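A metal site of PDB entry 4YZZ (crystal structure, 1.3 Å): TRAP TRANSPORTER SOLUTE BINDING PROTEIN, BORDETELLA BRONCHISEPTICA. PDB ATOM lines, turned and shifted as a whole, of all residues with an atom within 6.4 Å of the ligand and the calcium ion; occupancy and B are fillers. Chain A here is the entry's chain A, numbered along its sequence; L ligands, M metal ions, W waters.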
ATOM      1  N   TRP A  41      19.700  28.492 -12.582  1.00  0.00           N
ATOM      2  CA  TRP A  41      19.165  29.802 -13.011  1.00  0.00           C
ATOM      3  C   TRP A  41      19.574  30.968 -12.138  1.00  0.00           C
ATOM      4  O   TRP A  41      19.769  30.833 -10.936  1.00  0.00           O
ATOM      5  CB  TRP A  41      17.633  29.757 -13.003  1.00  0.00           C
ATOM      6  CG  TRP A  41      17.100  28.396 -13.188  1.00  0.00           C
ATOM      7  CD1 TRP A  41      16.357  27.687 -12.298  1.00  0.00           C
ATOM      8  CD2 TRP A  41      17.272  27.536 -14.340  1.00  0.00           C
ATOM      9  NE1 TRP A  41      16.068  26.450 -12.806  1.00  0.00           N
ATOM     10  CE2 TRP A  41      16.615  26.327 -14.055  1.00  0.00           C
ATOM     11  CE3 TRP A  41      17.933  27.666 -15.560  1.00  0.00           C
ATOM     12  CZ2 TRP A  41      16.608  25.260 -14.949  1.00  0.00           C
ATOM     13  CZ3 TRP A  41      17.916  26.609 -16.449  1.00  0.00           C
ATOM     14  CH2 TRP A  41      17.251  25.426 -16.149  1.00  0.00           C
ATOM     15  N   ILE A  48      11.229  30.903 -13.852  1.00  0.00           N
ATOM     16  CA  ILE A  48      11.831  29.579 -13.646  1.00  0.00           C
ATOM     17  C   ILE A  48      12.487  29.408 -12.261  1.00  0.00           C
ATOM     18  O   ILE A  48      12.246  28.392 -11.584  1.00  0.00           O
ATOM     19  CB  ILE A  48      12.773  29.199 -14.822  1.00  0.00           C
ATOM     20  CG1 ILE A  48      13.216  27.749 -14.738  1.00  0.00           C
ATOM     21  CG2 ILE A  48      13.961  30.141 -14.934  1.00  0.00           C
ATOM     22  CD1 ILE A  48      13.781  27.251 -16.062  1.00  0.00           C
ATOM     23  N   VAL A  97      16.888  21.796 -13.401  1.00  0.00           N
ATOM     24  CA  VAL A  97      17.754  21.882 -14.570  1.00  0.00           C
ATOM     25  C   VAL A  97      17.014  21.624 -15.886  1.00  0.00           C
ATOM     26  O   VAL A  97      15.885  21.138 -15.946  1.00  0.00           O
ATOM     27  CB  VAL A  97      18.919  20.842 -14.484  1.00  0.00           C
ATOM     28  CG1 VAL A  97      19.781  21.089 -13.244  1.00  0.00           C
ATOM     29  CG2 VAL A  97      18.402  19.397 -14.508  1.00  0.00           C
ATOM     30  N   LEU A  98      17.727  21.943 -16.958  1.00  0.00           N
ATOM     31  CA  LEU A  98      17.384  21.506 -18.294  1.00  0.00           C
ATOM     32  C   LEU A  98      18.210  20.262 -18.531  1.00  0.00           C
ATOM     33  O   LEU A  98      19.439  20.346 -18.649  1.00  0.00           O
ATOM     34  CB  LEU A  98      17.743  22.574 -19.314  1.00  0.00           C
ATOM     35  CG  LEU A  98      17.343  22.239 -20.759  1.00  0.00           C
ATOM     36  CD1 LEU A  98      15.956  22.791 -20.996  1.00  0.00           C
ATOM     37  CD2 LEU A  98      18.376  22.781 -21.776  1.00  0.00           C
ATOM     38  N   MET A 101      21.102  19.992 -21.052  1.00  0.00           N
ATOM     39  CA  MET A 101      22.433  20.553 -20.827  1.00  0.00           C
ATOM     40  C   MET A 101      23.459  19.425 -20.712  1.00  0.00           C
ATOM     41  O   MET A 101      24.633  19.592 -21.065  1.00  0.00           O
ATOM     42  CB  MET A 101      22.460  21.433 -19.576  1.00  0.00           C
ATOM     43  CG  MET A 101      23.823  22.086 -19.433  1.00  0.00           C
ATOM     44  SD  MET A 101      23.929  23.141 -17.993  1.00  0.00           S
ATOM     45  CE  MET A 101      25.443  24.025 -18.364  1.00  0.00           C
ATOM     46  N   VAL A 154       8.475  25.725 -19.963  1.00  0.00           N
ATOM     47  CA  VAL A 154       8.461  27.121 -20.386  1.00  0.00           C
ATOM     48  C   VAL A 154       7.684  27.321 -21.686  1.00  0.00           C
ATOM     49  O   VAL A 154       7.609  28.455 -22.208  1.00  0.00           O
ATOM     50  CB  VAL A 154       9.895  27.673 -20.516  1.00  0.00           C
ATOM     51  CG1 VAL A 154      10.713  27.339 -19.291  1.00  0.00           C
ATOM     52  CG2 VAL A 154      10.592  27.121 -21.744  1.00  0.00           C
ATOM     53  N   GLN A 157       9.606  28.164 -26.929  1.00  0.00           N
ATOM     54  CA  GLN A 157      10.565  29.240 -26.766  1.00  0.00           C
ATOM     55  C   GLN A 157      10.565  30.155 -27.975  1.00  0.00           C
ATOM     56  O   GLN A 157       9.991  29.842 -29.018  1.00  0.00           O
ATOM     57  CB  GLN A 157      11.938  28.625 -26.578  1.00  0.00           C
ATOM     58  CG  GLN A 157      12.035  27.806 -25.305  1.00  0.00           C
ATOM     59  CD  GLN A 157      13.206  26.895 -25.341  1.00  0.00           C
ATOM     60  OE1 GLN A 157      14.268  27.188 -24.762  1.00  0.00           O
ATOM     61  NE2 GLN A 157      13.056  25.770 -26.039  1.00  0.00           N
ATOM     62  N   MET A 158      11.183  31.330 -27.820  1.00  0.00           N
ATOM     63  CA  MET A 158      11.485  32.169 -28.976  1.00  0.00           C
ATOM     64  C   MET A 158      12.697  31.607 -29.734  1.00  0.00           C
ATOM     65  O   MET A 158      13.366  30.686 -29.254  1.00  0.00           O
ATOM     66  CB  MET A 158      11.696  33.615 -28.539  1.00  0.00           C
ATOM     67  CG  MET A 158      10.382  34.243 -28.100  1.00  0.00           C
ATOM     68  SD  MET A 158       9.222  34.514 -29.474  1.00  0.00           S
ATOM     69  CE  MET A 158       9.922  35.985 -30.252  1.00  0.00           C
ATOM     70  N   ARG A 178      24.793  30.882 -29.002  1.00  0.00           N
ATOM     71  CA  ARG A 178      24.444  30.230 -27.742  1.00  0.00           C
ATOM     72  C   ARG A 178      23.064  29.613 -27.865  1.00  0.00           C
ATOM     73  O   ARG A 178      22.094  30.278 -28.207  1.00  0.00           O
ATOM     74  CB  ARG A 178      24.438  31.252 -26.609  1.00  0.00           C
ATOM     75  CG  ARG A 178      24.230  30.659 -25.209  1.00  0.00           C
ATOM     76  CD  ARG A 178      22.783  30.496 -24.810  1.00  0.00           C
ATOM     77  NE  ARG A 178      22.738  29.616 -23.654  1.00  0.00           N
ATOM     78  CZ  ARG A 178      21.701  28.887 -23.289  1.00  0.00           C
ATOM     79  NH1 ARG A 178      20.543  28.943 -23.918  1.00  0.00           N
ATOM     80  NH2 ARG A 178      21.828  28.084 -22.247  1.00  0.00           N
ATOM     81  N   ILE A 179      22.982  28.331 -27.546  1.00  0.00           N
ATOM     82  CA  ILE A 179      21.699  27.622 -27.563  1.00  0.00           C
ATOM     83  C   ILE A 179      21.815  26.452 -26.606  1.00  0.00           C
ATOM     84  O   ILE A 179      22.802  25.723 -26.612  1.00  0.00           O
ATOM     85  CB  ILE A 179      21.327  27.154 -29.002  1.00  0.00           C
ATOM     86  CG1 ILE A 179      20.094  26.239 -28.970  1.00  0.00           C
ATOM     87  CG2 ILE A 179      22.485  26.481 -29.701  1.00  0.00           C
ATOM     88  CD1 ILE A 179      19.502  25.928 -30.351  1.00  0.00           C
ATOM     89  N   GLY A 180      20.795  26.294 -25.771  1.00  0.00           N
ATOM     90  CA  GLY A 180      20.714  25.150 -24.875  1.00  0.00           C
ATOM     91  C   GLY A 180      19.936  24.007 -25.501  1.00  0.00           C
ATOM     92  O   GLY A 180      19.083  24.221 -26.359  1.00  0.00           O
ATOM     93  N   GLY A 181      20.228  22.787 -25.078  1.00  0.00           N
ATOM     94  CA  GLY A 181      19.470  21.627 -25.481  1.00  0.00           C
ATOM     95  C   GLY A 181      19.871  20.991 -26.807  1.00  0.00           C
ATOM     96  O   GLY A 181      20.910  21.317 -27.416  1.00  0.00           O
ATOM     97  N   GLN A 196      26.329  25.751 -25.151  1.00  0.00           N
ATOM     98  CA  GLN A 196      25.372  25.844 -24.038  1.00  0.00           C
ATOM     99  C   GLN A 196      25.885  26.731 -22.878  1.00  0.00           C
ATOM    100  O   GLN A 196      25.953  26.305 -21.739  1.00  0.00           O
ATOM    101  CB  GLN A 196      24.998  24.436 -23.506  1.00  0.00           C
ATOM    102  CG  GLN A 196      24.428  23.508 -24.569  1.00  0.00           C
ATOM    103  CD  GLN A 196      23.420  22.516 -24.017  1.00  0.00           C
ATOM    104  OE1 GLN A 196      22.493  22.896 -23.280  1.00  0.00           O
ATOM    105  NE2 GLN A 196      23.585  21.263 -24.354  1.00  0.00           N
ATOM    106  N   ILE A 197      26.194  27.977 -23.184  1.00  0.00           N
ATOM    107  CA  ILE A 197      26.738  28.912 -22.190  1.00  0.00           C
ATOM    108  C   ILE A 197      25.647  29.160 -21.127  1.00  0.00           C
ATOM    109  O   ILE A 197      24.483  29.374 -21.469  1.00  0.00           O
ATOM    110  CB  ILE A 197      27.160  30.233 -22.895  1.00  0.00           C
ATOM    111  CG1 ILE A 197      28.350  30.009 -23.853  1.00  0.00           C
ATOM    112  CG2 ILE A 197      27.507  31.328 -21.873  1.00  0.00           C
ATOM    113  CD1 ILE A 197      28.510  31.083 -24.898  1.00  0.00           C
ATOM    114  N   PRO A 199      23.062  30.783 -18.319  1.00  0.00           N
ATOM    115  CA  PRO A 199      22.271  32.008 -18.530  1.00  0.00           C
ATOM    116  C   PRO A 199      22.960  33.295 -18.118  1.00  0.00           C
ATOM    117  O   PRO A 199      22.888  34.268 -18.861  1.00  0.00           O
ATOM    118  CB  PRO A 199      21.012  31.782 -17.687  1.00  0.00           C
ATOM    119  CG  PRO A 199      21.259  30.552 -16.903  1.00  0.00           C
ATOM    120  CD  PRO A 199      22.266  29.742 -17.649  1.00  0.00           C
ATOM    121  N   GLU A 215      19.932  32.264 -28.023  1.00  0.00           N
ATOM    122  CA  GLU A 215      18.565  32.014 -27.562  1.00  0.00           C
ATOM    123  C   GLU A 215      18.647  31.655 -26.083  1.00  0.00           C
ATOM    124  O   GLU A 215      19.631  31.080 -25.618  1.00  0.00           O
ATOM    125  CB  GLU A 215      17.907  30.894 -28.384  1.00  0.00           C
ATOM    126  CG  GLU A 215      18.407  29.484 -28.098  1.00  0.00           C
ATOM    127  CD  GLU A 215      17.735  28.798 -26.899  1.00  0.00           C
ATOM    128  OE1 GLU A 215      16.507  28.981 -26.662  1.00  0.00           O
ATOM    129  OE2 GLU A 215      18.423  28.051 -26.202  1.00  0.00           O
ATOM    130  N   TRP A 216      17.601  32.041 -25.342  1.00  0.00           N
ATOM    131  CA  TRP A 216      17.461  31.640 -23.941  1.00  0.00           C
ATOM    132  C   TRP A 216      16.087  30.990 -23.770  1.00  0.00           C
ATOM    133  O   TRP A 216      16.023  29.757 -23.816  1.00  0.00           O
ATOM    134  CB  TRP A 216      17.727  32.814 -22.985  1.00  0.00           C
ATOM    135  CG  TRP A 216      17.333  32.490 -21.586  1.00  0.00           C
ATOM    136  CD1 TRP A 216      16.336  33.075 -20.854  1.00  0.00           C
ATOM    137  CD2 TRP A 216      17.877  31.438 -20.765  1.00  0.00           C
ATOM    138  NE1 TRP A 216      16.232  32.457 -19.622  1.00  0.00           N
ATOM    139  CE2 TRP A 216      17.160  31.453 -19.548  1.00  0.00           C
ATOM    140  CE3 TRP A 216      18.890  30.484 -20.946  1.00  0.00           C
ATOM    141  CZ2 TRP A 216      17.429  30.552 -18.515  1.00  0.00           C
ATOM    142  CZ3 TRP A 216      19.152  29.616 -19.928  1.00  0.00           C
ATOM    143  CH2 TRP A 216      18.437  29.650 -18.724  1.00  0.00           C
ATOM    144  N   ILE A 217      15.019  31.779 -23.598  1.00  0.00           N
ATOM    145  CA  ILE A 217      13.672  31.227 -23.379  1.00  0.00           C
ATOM    146  C   ILE A 217      12.544  31.988 -24.085  1.00  0.00           C
ATOM    147  O   ILE A 217      11.775  31.411 -24.870  1.00  0.00           O
ATOM    148  CB  ILE A 217      13.337  31.139 -21.874  1.00  0.00           C
ATOM    149  CG1 ILE A 217      14.240  30.111 -21.180  1.00  0.00           C
ATOM    150  CG2 ILE A 217      11.885  30.737 -21.682  1.00  0.00           C
ATOM    151  CD1 ILE A 217      13.987  29.939 -19.681  1.00  0.00           C
ATOM    152  N   PHE A 240      13.511  24.470 -31.322  1.00  0.00           N
ATOM    153  CA  PHE A 240      14.560  23.713 -30.632  1.00  0.00           C
ATOM    154  C   PHE A 240      14.049  22.571 -29.785  1.00  0.00           C
ATOM    155  O   PHE A 240      14.630  21.494 -29.740  1.00  0.00           O
ATOM    156  CB  PHE A 240      15.382  24.678 -29.745  1.00  0.00           C
ATOM    157  CG  PHE A 240      15.702  26.001 -30.401  1.00  0.00           C
ATOM    158  CD1 PHE A 240      16.166  26.041 -31.701  1.00  0.00           C
ATOM    159  CD2 PHE A 240      15.510  27.218 -29.739  1.00  0.00           C
ATOM    160  CE1 PHE A 240      16.455  27.265 -32.324  1.00  0.00           C
ATOM    161  CE2 PHE A 240      15.799  28.433 -30.367  1.00  0.00           C
ATOM    162  CZ  PHE A 240      16.269  28.441 -31.651  1.00  0.00           C
ATOM    163  N   GLU A 241      12.944  22.836 -29.108  1.00  0.00           N
ATOM    164  CA  GLU A 241      12.139  21.822 -28.423  1.00  0.00           C
ATOM    165  C   GLU A 241      10.681  22.123 -28.718  1.00  0.00           C
ATOM    166  O   GLU A 241      10.303  23.275 -28.876  1.00  0.00           O
ATOM    167  CB  GLU A 241      12.339  21.868 -26.896  1.00  0.00           C
ATOM    168  CG  GLU A 241      13.675  21.321 -26.383  1.00  0.00           C
ATOM    169  CD  GLU A 241      14.832  22.313 -26.319  1.00  0.00           C
ATOM    170  OE1 GLU A 241      14.639  23.561 -26.346  1.00  0.00           O
ATOM    171  OE2 GLU A 241      15.979  21.834 -26.236  1.00  0.00           O
ATOM    172  N   ALA A 244      10.148  23.224 -23.719  1.00  0.00           N
ATOM    173  CA  ALA A 244      11.294  22.929 -22.859  1.00  0.00           C
ATOM    174  C   ALA A 244      10.818  22.586 -21.456  1.00  0.00           C
ATOM    175  O   ALA A 244      10.408  23.451 -20.681  1.00  0.00           O
ATOM    176  CB  ALA A 244      12.297  24.083 -22.854  1.00  0.00           C
ATOM    177  N   SER A 245      10.867  21.298 -21.163  1.00  0.00           N
ATOM    178  CA  SER A 245      10.447  20.764 -19.877  1.00  0.00           C
ATOM    179  C   SER A 245      11.612  20.811 -18.910  1.00  0.00           C
ATOM    180  O   SER A 245      12.774  20.616 -19.298  1.00  0.00           O
ATOM    181  CB  SER A 245       9.948  19.328 -20.079  1.00  0.00           C
ATOM    182  OG  SER A 245       9.391  18.795 -18.897  1.00  0.00           O
ATOM    183  N   ILE A 246      11.303  21.118 -17.649  1.00  0.00           N
ATOM    184  CA  ILE A 246      12.283  21.275 -16.589  1.00  0.00           C
ATOM    185  C   ILE A 246      12.237  20.081 -15.649  1.00  0.00           C
ATOM    186  O   ILE A 246      11.153  19.576 -15.345  1.00  0.00           O
ATOM    187  CB  ILE A 246      12.026  22.578 -15.826  1.00  0.00           C
ATOM    188  CG1 ILE A 246      11.882  23.764 -16.788  1.00  0.00           C
ATOM    189  CG2 ILE A 246      13.097  22.831 -14.783  1.00  0.00           C
ATOM    190  CD1 ILE A 246      13.096  24.026 -17.707  1.00  0.00           C
ATOM    191  N   TYR A 281       4.789  31.989 -16.860  1.00  0.00           N
ATOM    192  CA  TYR A 281       5.288  32.405 -18.172  1.00  0.00           C
ATOM    193  C   TYR A 281       4.163  32.904 -19.087  1.00  0.00           C
ATOM    194  O   TYR A 281       4.257  33.979 -19.709  1.00  0.00           O
ATOM    195  CB  TYR A 281       6.019  31.252 -18.852  1.00  0.00           C
ATOM    196  CG  TYR A 281       7.480  31.124 -18.456  1.00  0.00           C
ATOM    197  CD1 TYR A 281       8.399  32.106 -18.802  1.00  0.00           C
ATOM    198  CD2 TYR A 281       7.934  30.036 -17.722  1.00  0.00           C
ATOM    199  CE1 TYR A 281       9.734  32.006 -18.460  1.00  0.00           C
ATOM    200  CE2 TYR A 281       9.267  29.927 -17.363  1.00  0.00           C
ATOM    201  CZ  TYR A 281      10.157  30.916 -17.718  1.00  0.00           C
ATOM    202  OH  TYR A 281      11.467  30.773 -17.357  1.00  0.00           O
HETATM  203  C1  LIG L   1      17.170  26.750 -21.450  1.00  0.00           C
HETATM  204  C2  LIG L   1      14.792  26.705 -21.693  1.00  0.00           C
HETATM  205  C3  LIG L   1      14.646  26.425 -20.339  1.00  0.00           C
HETATM  206  C4  LIG L   1      18.411  26.867 -22.103  1.00  0.00           C
HETATM  207  C5  LIG L   1      15.760  26.302 -19.532  1.00  0.00           C
HETATM  208  C6  LIG L   1      17.046  26.395 -20.091  1.00  0.00           C
HETATM  209  O1  LIG L   1      18.419  27.219 -23.324  1.00  0.00           O
HETATM  210  O2  LIG L   1      19.483  26.513 -21.549  1.00  0.00           O
HETATM  211  N1  LIG L   1      16.065  26.879 -22.229  1.00  0.00           N
HETATM  212 CA    CA M   1      16.483  27.599 -24.648  1.00  0.00          CA
HETATM  213  O   HOH W   1      21.573  24.630 -21.148  1.00  0.00           O
HETATM  214  O   HOH W   2      16.643  25.449 -25.735  1.00  0.00           O
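Water W2 lies within hydrogen-bond range of the backbone carbonyl oxygen of Gly 180 (2.8 Å) and the side-chain carboxylate of Glu 241 (2.8 Å). Water W1 bridges O2 of the ligand (2.8 Å) and OE1 of Gln 196 (2.9 Å).
O of Glu 215 sits at hydrogen-bond distance from NH1 of Arg 178. The backbone carbonyl oxygen (O) of Ile 217 sits at hydrogen-bond distance from the backbone NH (N) of Met 158 (3.0 Å). OE2 of Glu 215 lies close to N of Gly 180 (3.0 Å). NE of Arg 178 is in hydrogen-bond range of O of Ile 197 (2.8 Å). The side-chain carboxylate (OE1) of Glu 241 lies within hydrogen-bond range of the side-chain amide nitrogen (NE2) of Gln 157, at 2.7 Å. The backbone carbonyl oxygen of Ala 244 sits at hydrogen-bond distance from the backbone NH of Val 154 (3.1 Å).
The guanidinium group (NH2) of Arg 178 is in salt-bridge range of an oxygen (O2) of the ligand (2.9 Å).
The calcium ion is bound by the side-chain amide oxygen (OE1) of Gln 157 (2.3 Å), the backbone carbonyl oxygen (O) of Trp 216 (2.4 Å), an oxygen (O1) of the ligand (2.4 Å), water W2 (2.4 Å), the side-chain carboxylate (OE1) of Glu 215 (2.4 Å), the side-chain carboxylate (OE2) of Glu 215 (2.5 Å) and a nitrogen (N1) of the ligand (2.6 Å). The calcium ion has seven donor atoms within binding distance.
Merely in contact with the ligand: Trp 41, Leu 98, Gly 180, Ile 217, Ala 244 and Ile 246. Hydrophobic or aromatic side chains within 4 Å of the ligand: Trp 41, Leu 98, Trp 216, Ile 217, Ala 244 and Ile 246. Of the 24 residues printed, 10 come within 4 Å of the ligand.
Within 4 Å of the calcium ion: Gln 157, Glu 215 and Trp 216.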
